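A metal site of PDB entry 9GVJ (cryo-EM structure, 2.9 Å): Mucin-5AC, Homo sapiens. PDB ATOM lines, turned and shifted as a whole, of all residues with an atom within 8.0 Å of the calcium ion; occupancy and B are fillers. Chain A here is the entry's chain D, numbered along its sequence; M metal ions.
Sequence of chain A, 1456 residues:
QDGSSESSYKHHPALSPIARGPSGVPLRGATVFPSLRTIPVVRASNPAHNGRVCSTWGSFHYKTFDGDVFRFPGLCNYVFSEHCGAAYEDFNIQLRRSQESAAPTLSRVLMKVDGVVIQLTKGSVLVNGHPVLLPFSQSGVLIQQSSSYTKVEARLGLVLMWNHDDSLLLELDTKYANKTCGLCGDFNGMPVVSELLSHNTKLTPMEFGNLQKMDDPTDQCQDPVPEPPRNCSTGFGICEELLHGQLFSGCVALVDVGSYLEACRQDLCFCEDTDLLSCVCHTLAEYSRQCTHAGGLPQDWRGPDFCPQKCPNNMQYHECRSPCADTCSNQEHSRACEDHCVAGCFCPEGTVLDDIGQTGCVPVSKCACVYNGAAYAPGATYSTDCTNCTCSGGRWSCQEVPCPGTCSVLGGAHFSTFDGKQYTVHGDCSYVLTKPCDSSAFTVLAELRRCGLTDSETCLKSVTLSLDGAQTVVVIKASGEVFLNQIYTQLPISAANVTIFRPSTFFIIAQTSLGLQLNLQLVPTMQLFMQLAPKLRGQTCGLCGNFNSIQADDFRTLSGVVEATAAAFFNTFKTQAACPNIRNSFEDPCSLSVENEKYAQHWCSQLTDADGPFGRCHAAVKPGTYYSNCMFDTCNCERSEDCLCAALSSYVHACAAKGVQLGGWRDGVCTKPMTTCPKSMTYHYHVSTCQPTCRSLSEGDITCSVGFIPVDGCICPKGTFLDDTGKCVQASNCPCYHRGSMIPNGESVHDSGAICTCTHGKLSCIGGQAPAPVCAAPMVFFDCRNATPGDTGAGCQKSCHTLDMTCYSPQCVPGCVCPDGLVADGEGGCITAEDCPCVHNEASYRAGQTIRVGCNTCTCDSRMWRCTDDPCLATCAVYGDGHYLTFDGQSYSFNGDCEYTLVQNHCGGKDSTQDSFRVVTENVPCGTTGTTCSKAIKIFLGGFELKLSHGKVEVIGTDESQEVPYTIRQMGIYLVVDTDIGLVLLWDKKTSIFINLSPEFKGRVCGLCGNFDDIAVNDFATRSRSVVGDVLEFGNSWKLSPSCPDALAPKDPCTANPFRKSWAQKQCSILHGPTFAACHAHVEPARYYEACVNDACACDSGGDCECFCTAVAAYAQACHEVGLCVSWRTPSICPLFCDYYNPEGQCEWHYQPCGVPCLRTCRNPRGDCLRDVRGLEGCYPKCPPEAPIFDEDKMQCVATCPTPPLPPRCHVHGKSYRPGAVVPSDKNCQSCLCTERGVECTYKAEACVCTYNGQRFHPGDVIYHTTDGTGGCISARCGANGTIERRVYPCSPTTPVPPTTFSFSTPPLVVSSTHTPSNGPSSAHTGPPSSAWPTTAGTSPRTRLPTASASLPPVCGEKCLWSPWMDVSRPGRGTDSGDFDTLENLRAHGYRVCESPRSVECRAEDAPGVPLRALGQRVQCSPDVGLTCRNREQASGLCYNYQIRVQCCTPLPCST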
ATOM      1  N   THR A 886      -8.193  -5.891  -5.143  1.00  0.00           N
ATOM      2  CA  THR A 886      -8.604  -6.370  -3.829  1.00  0.00           C
ATOM      3  C   THR A 886      -9.785  -5.560  -3.302  1.00  0.00           C
ATOM      4  O   THR A 886     -10.303  -4.657  -3.953  1.00  0.00           O
ATOM      5  CB  THR A 886      -7.428  -6.316  -2.864  1.00  0.00           C
ATOM      6  OG1 THR A 886      -7.031  -4.955  -2.663  1.00  0.00           O
ATOM      7  CG2 THR A 886      -6.242  -7.103  -3.410  1.00  0.00           C
ATOM      8  N   PHE A 887     -10.214  -5.913  -2.077  1.00  0.00           N
ATOM      9  CA  PHE A 887     -11.307  -5.189  -1.435  1.00  0.00           C
ATOM     10  C   PHE A 887     -10.919  -3.744  -1.164  1.00  0.00           C
ATOM     11  O   PHE A 887     -11.740  -2.838  -1.338  1.00  0.00           O
ATOM     12  CB  PHE A 887     -11.704  -5.888  -0.132  1.00  0.00           C
ATOM     13  CG  PHE A 887     -12.425  -7.190  -0.335  1.00  0.00           C
ATOM     14  CD1 PHE A 887     -13.702  -7.205  -0.866  1.00  0.00           C
ATOM     15  CD2 PHE A 887     -11.834  -8.393   0.023  1.00  0.00           C
ATOM     16  CE1 PHE A 887     -14.370  -8.398  -1.044  1.00  0.00           C
ATOM     17  CE2 PHE A 887     -12.495  -9.585  -0.162  1.00  0.00           C
ATOM     18  CZ  PHE A 887     -13.773  -9.589  -0.693  1.00  0.00           C
ATOM     19  N   ASP A 888      -9.688  -3.516  -0.729  1.00  0.00           N
ATOM     20  CA  ASP A 888      -9.219  -2.200  -0.331  1.00  0.00           C
ATOM     21  C   ASP A 888      -8.711  -1.371  -1.500  1.00  0.00           C
ATOM     22  O   ASP A 888      -8.280  -0.229  -1.289  1.00  0.00           O
ATOM     23  CB  ASP A 888      -8.132  -2.320   0.731  1.00  0.00           C
ATOM     24  CG  ASP A 888      -8.651  -2.888   2.042  1.00  0.00           C
ATOM     25  OD1 ASP A 888      -9.873  -2.784   2.289  1.00  0.00           O
ATOM     26  OD2 ASP A 888      -7.850  -3.439   2.814  1.00  0.00           O
ATOM     27  N   GLY A 889      -8.748  -1.909  -2.718  1.00  0.00           N
ATOM     28  CA  GLY A 889      -8.340  -1.167  -3.896  1.00  0.00           C
ATOM     29  C   GLY A 889      -6.934  -1.424  -4.386  1.00  0.00           C
ATOM     30  O   GLY A 889      -6.463  -0.696  -5.266  1.00  0.00           O
ATOM     31  N   GLN A 890      -6.252  -2.433  -3.854  1.00  0.00           N
ATOM     32  CA  GLN A 890      -4.905  -2.774  -4.309  1.00  0.00           C
ATOM     33  C   GLN A 890      -5.017  -3.583  -5.601  1.00  0.00           C
ATOM     34  O   GLN A 890      -5.578  -4.680  -5.612  1.00  0.00           O
ATOM     35  CB  GLN A 890      -4.155  -3.561  -3.239  1.00  0.00           C
ATOM     36  CG  GLN A 890      -2.806  -4.096  -3.682  1.00  0.00           C
ATOM     37  CD  GLN A 890      -1.799  -3.006  -3.925  1.00  0.00           C
ATOM     38  OE1 GLN A 890      -1.268  -2.870  -5.024  1.00  0.00           O
ATOM     39  NE2 GLN A 890      -1.510  -2.218  -2.894  1.00  0.00           N
ATOM     40  N   GLY A1003     -11.681  -6.781   8.303  1.00  0.00           N
ATOM     41  CA  GLY A1003     -10.636  -7.308   9.146  1.00  0.00           C
ATOM     42  C   GLY A1003     -10.753  -8.777   9.474  1.00  0.00           C
ATOM     43  O   GLY A1003      -9.952  -9.289  10.270  1.00  0.00           O
ATOM     44  N   VAL A1005     -11.328 -11.313   6.849  1.00  0.00           N
ATOM     45  CA  VAL A1005     -11.067 -12.152   5.691  1.00  0.00           C
ATOM     46  C   VAL A1005      -9.585 -12.072   5.337  1.00  0.00           C
ATOM     47  O   VAL A1005      -8.843 -11.216   5.815  1.00  0.00           O
ATOM     48  CB  VAL A1005     -11.944 -11.752   4.493  1.00  0.00           C
ATOM     49  CG1 VAL A1005     -13.401 -12.066   4.784  1.00  0.00           C
ATOM     50  CG2 VAL A1005     -11.776 -10.285   4.173  1.00  0.00           C
ATOM     51  N   CYS A1009      -7.549 -11.743  -2.131  1.00  0.00           N
ATOM     52  CA  CYS A1009      -8.396 -10.562  -2.234  1.00  0.00           C
ATOM     53  C   CYS A1009      -8.112  -9.537  -1.133  1.00  0.00           C
ATOM     54  O   CYS A1009      -8.856  -8.551  -1.016  1.00  0.00           O
ATOM     55  CB  CYS A1009      -9.867 -10.960  -2.198  1.00  0.00           C
ATOM     56  SG  CYS A1009     -10.583 -11.282  -3.822  1.00  0.00           S
ATOM     57  N   GLY A1010      -7.087  -9.749  -0.321  1.00  0.00           N
ATOM     58  CA  GLY A1010      -6.773  -8.818   0.743  1.00  0.00           C
ATOM     59  C   GLY A1010      -7.458  -9.199   2.046  1.00  0.00           C
ATOM     60  O   GLY A1010      -7.997 -10.288   2.219  1.00  0.00           O
ATOM     61  N   ASN A1011      -7.422  -8.242   2.986  1.00  0.00           N
ATOM     62  CA  ASN A1011      -7.970  -8.460   4.312  1.00  0.00           C
ATOM     63  C   ASN A1011      -9.090  -7.506   4.689  1.00  0.00           C
ATOM     64  O   ASN A1011      -9.639  -7.624   5.789  1.00  0.00           O
ATOM     65  CB  ASN A1011      -6.845  -8.370   5.364  1.00  0.00           C
ATOM     66  CG  ASN A1011      -6.581  -6.950   5.809  1.00  0.00           C
ATOM     67  OD1 ASN A1011      -7.132  -6.502   6.815  1.00  0.00           O
ATOM     68  ND2 ASN A1011      -5.723  -6.251   5.076  1.00  0.00           N
ATOM     69  N   PHE A1012      -9.462  -6.570   3.802  1.00  0.00           N
ATOM     70  CA  PHE A1012     -10.639  -5.710   3.978  1.00  0.00           C
ATOM     71  C   PHE A1012     -10.535  -4.904   5.276  1.00  0.00           C
ATOM     72  O   PHE A1012     -11.314  -5.067   6.212  1.00  0.00           O
ATOM     73  CB  PHE A1012     -11.913  -6.558   3.945  1.00  0.00           C
ATOM     74  CG  PHE A1012     -13.178  -5.746   3.782  1.00  0.00           C
ATOM     75  CD1 PHE A1012     -13.141  -4.382   3.578  1.00  0.00           C
ATOM     76  CD2 PHE A1012     -14.420  -6.373   3.852  1.00  0.00           C
ATOM     77  CE1 PHE A1012     -14.307  -3.657   3.438  1.00  0.00           C
ATOM     78  CE2 PHE A1012     -15.584  -5.659   3.712  1.00  0.00           C
ATOM     79  CZ  PHE A1012     -15.533  -4.292   3.508  1.00  0.00           C
ATOM     80  N   ASP A1013      -9.549  -4.001   5.302  1.00  0.00           N
ATOM     81  CA  ASP A1013      -9.412  -3.095   6.438  1.00  0.00           C
ATOM     82  C   ASP A1013      -9.132  -1.669   5.975  1.00  0.00           C
ATOM     83  O   ASP A1013      -8.519  -0.875   6.700  1.00  0.00           O
ATOM     84  CB  ASP A1013      -8.317  -3.551   7.394  1.00  0.00           C
ATOM     85  CG  ASP A1013      -6.925  -3.436   6.794  1.00  0.00           C
ATOM     86  OD1 ASP A1013      -6.786  -3.640   5.580  1.00  0.00           O
ATOM     87  OD2 ASP A1013      -5.974  -3.138   7.555  1.00  0.00           O
ATOM     88  N   ASP A1014      -9.569  -1.327   4.753  1.00  0.00           N
ATOM     89  CA  ASP A1014      -9.478   0.008   4.143  1.00  0.00           C
ATOM     90  C   ASP A1014      -8.050   0.422   3.817  1.00  0.00           C
ATOM     91  O   ASP A1014      -7.857   1.514   3.281  1.00  0.00           O
ATOM     92  CB  ASP A1014     -10.127   1.091   5.017  1.00  0.00           C
ATOM     93  CG  ASP A1014     -11.642   1.026   5.001  1.00  0.00           C
ATOM     94  OD1 ASP A1014     -12.188  -0.089   4.854  1.00  0.00           O
ATOM     95  OD2 ASP A1014     -12.285   2.088   5.142  1.00  0.00           O
ATOM     96  N   ILE A1015      -7.054  -0.394   4.123  1.00  0.00           N
ATOM     97  CA  ILE A1015      -5.658  -0.101   3.836  1.00  0.00           C
ATOM     98  C   ILE A1015      -5.197  -1.033   2.730  1.00  0.00           C
ATOM     99  O   ILE A1015      -5.290  -2.259   2.866  1.00  0.00           O
ATOM    100  CB  ILE A1015      -4.774  -0.250   5.091  1.00  0.00           C
ATOM    101  CG1 ILE A1015      -5.355   0.578   6.234  1.00  0.00           C
ATOM    102  CG2 ILE A1015      -3.360   0.200   4.788  1.00  0.00           C
ATOM    103  CD1 ILE A1015      -4.575   0.449   7.531  1.00  0.00           C
ATOM    104  N   ALA A1016      -4.714  -0.468   1.631  1.00  0.00           N
ATOM    105  CA  ALA A1016      -4.359  -1.260   0.450  1.00  0.00           C
ATOM    106  C   ALA A1016      -2.908  -1.723   0.455  1.00  0.00           C
ATOM    107  O   ALA A1016      -2.570  -2.632  -0.318  1.00  0.00           O
ATOM    108  CB  ALA A1016      -4.619  -0.447  -0.821  1.00  0.00           C
ATOM    109  N   VAL A1017      -2.047  -1.151   1.294  1.00  0.00           N
ATOM    110  CA  VAL A1017      -0.638  -1.526   1.249  1.00  0.00           C
ATOM    111  C   VAL A1017      -0.382  -2.826   2.010  1.00  0.00           C
ATOM    112  O   VAL A1017       0.575  -3.538   1.700  1.00  0.00           O
ATOM    113  CB  VAL A1017       0.242  -0.387   1.781  1.00  0.00           C
ATOM    114  CG1 VAL A1017       0.132   0.838   0.875  1.00  0.00           C
ATOM    115  CG2 VAL A1017      -0.136  -0.036   3.209  1.00  0.00           C
ATOM    116  N   ASN A1018      -1.209  -3.143   2.989  1.00  0.00           N
ATOM    117  CA  ASN A1018      -1.064  -4.381   3.753  1.00  0.00           C
ATOM    118  C   ASN A1018      -1.868  -5.534   3.178  1.00  0.00           C
ATOM    119  O   ASN A1018      -1.946  -6.603   3.796  1.00  0.00           O
ATOM    120  CB  ASN A1018      -1.439  -4.145   5.227  1.00  0.00           C
ATOM    121  CG  ASN A1018      -2.873  -3.695   5.414  1.00  0.00           C
ATOM    122  OD1 ASN A1018      -3.698  -3.808   4.507  1.00  0.00           O
ATOM    123  ND2 ASN A1018      -3.177  -3.169   6.595  1.00  0.00           N
ATOM    124  N   ASP A1019      -2.498  -5.340   2.011  1.00  0.00           N
ATOM    125  CA  ASP A1019      -3.234  -6.415   1.366  1.00  0.00           C
ATOM    126  C   ASP A1019      -2.327  -7.525   0.843  1.00  0.00           C
ATOM    127  O   ASP A1019      -2.837  -8.584   0.453  1.00  0.00           O
ATOM    128  CB  ASP A1019      -4.067  -5.849   0.211  1.00  0.00           C
ATOM    129  CG  ASP A1019      -5.445  -5.400   0.661  1.00  0.00           C
ATOM    130  OD1 ASP A1019      -5.743  -5.496   1.867  1.00  0.00           O
ATOM    131  OD2 ASP A1019      -6.227  -4.951  -0.204  1.00  0.00           O
ATOM    132  N   PHE A1020      -1.014  -7.307   0.817  1.00  0.00           N
ATOM    133  CA  PHE A1020      -0.061  -8.314   0.369  1.00  0.00           C
ATOM    134  C   PHE A1020       0.367  -9.250   1.505  1.00  0.00           C
ATOM    135  O   PHE A1020       1.436  -9.860   1.411  1.00  0.00           O
ATOM    136  CB  PHE A1020       1.170  -7.644  -0.245  1.00  0.00           C
ATOM    137  CG  PHE A1020       0.995  -7.282  -1.688  1.00  0.00           C
ATOM    138  CD1 PHE A1020      -0.171  -7.591  -2.369  1.00  0.00           C
ATOM    139  CD2 PHE A1020       2.009  -6.623  -2.371  1.00  0.00           C
ATOM    140  CE1 PHE A1020      -0.324  -7.255  -3.692  1.00  0.00           C
ATOM    141  CE2 PHE A1020       1.854  -6.277  -3.693  1.00  0.00           C
ATOM    142  CZ  PHE A1020       0.689  -6.597  -4.362  1.00  0.00           C
ATOM    143  N   ALA A1021      -0.433  -9.355   2.552  1.00  0.00           N
ATOM    144  CA  ALA A1021      -0.117 -10.256   3.653  1.00  0.00           C
ATOM    145  C   ALA A1021      -0.161 -11.698   3.169  1.00  0.00           C
ATOM    146  O   ALA A1021      -1.130 -12.131   2.530  1.00  0.00           O
ATOM    147  CB  ALA A1021      -1.084 -10.061   4.807  1.00  0.00           C
ATOM    148  N   VAL A1027       3.283  -9.073   5.746  1.00  0.00           N
ATOM    149  CA  VAL A1027       3.126  -8.249   4.541  1.00  0.00           C
ATOM    150  C   VAL A1027       4.476  -8.202   3.821  1.00  0.00           C
ATOM    151  O   VAL A1027       5.499  -7.826   4.398  1.00  0.00           O
ATOM    152  CB  VAL A1027       2.641  -6.832   4.892  1.00  0.00           C
ATOM    153  CG1 VAL A1027       2.804  -5.905   3.696  1.00  0.00           C
ATOM    154  CG2 VAL A1027       1.199  -6.873   5.356  1.00  0.00           C
HETATM  155 CA    CA M   1      -5.800  -4.294   3.728  1.00  0.00          CA
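The calcium ion is bound by OD1 of Asp 1013 (2.2 Å), OD1 of Asp 1019 (2.2 Å), O of Ile 1015 (2.3 Å), OD1 of Asn 1018 (2.3 Å), ND2 of Asn 1011 (2.4 Å) and OD2 of Asp 888 (2.4 Å).
The side-chain carboxylate (OD2) of Asp 1019 sits at hydrogen-bond distance from the side-chain hydroxyl (OG1) of Thr 886, at 2.6 Å.
The backbone carbonyl oxygen (O) of Asn 1011 is in hydrogen-bond range of the backbone NH (N) of Gly 1003, 3.3 Å away.
N of Asp 1014 is in hydrogen-bond range of OD1 of Asp 888 (2.9 Å).
Six residues have an atom within 4 Å of the calcium ion: Asp 888, Asn 1011, Asp 1013, Ile 1015, Asn 1018 and Asp 1019.
Along chain A the residues within 4 Å of the calcium ion span positions 888 to 1019.
The nearest printed residue that does not touch the calcium ion is Phe 1012 (4.3 Å).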
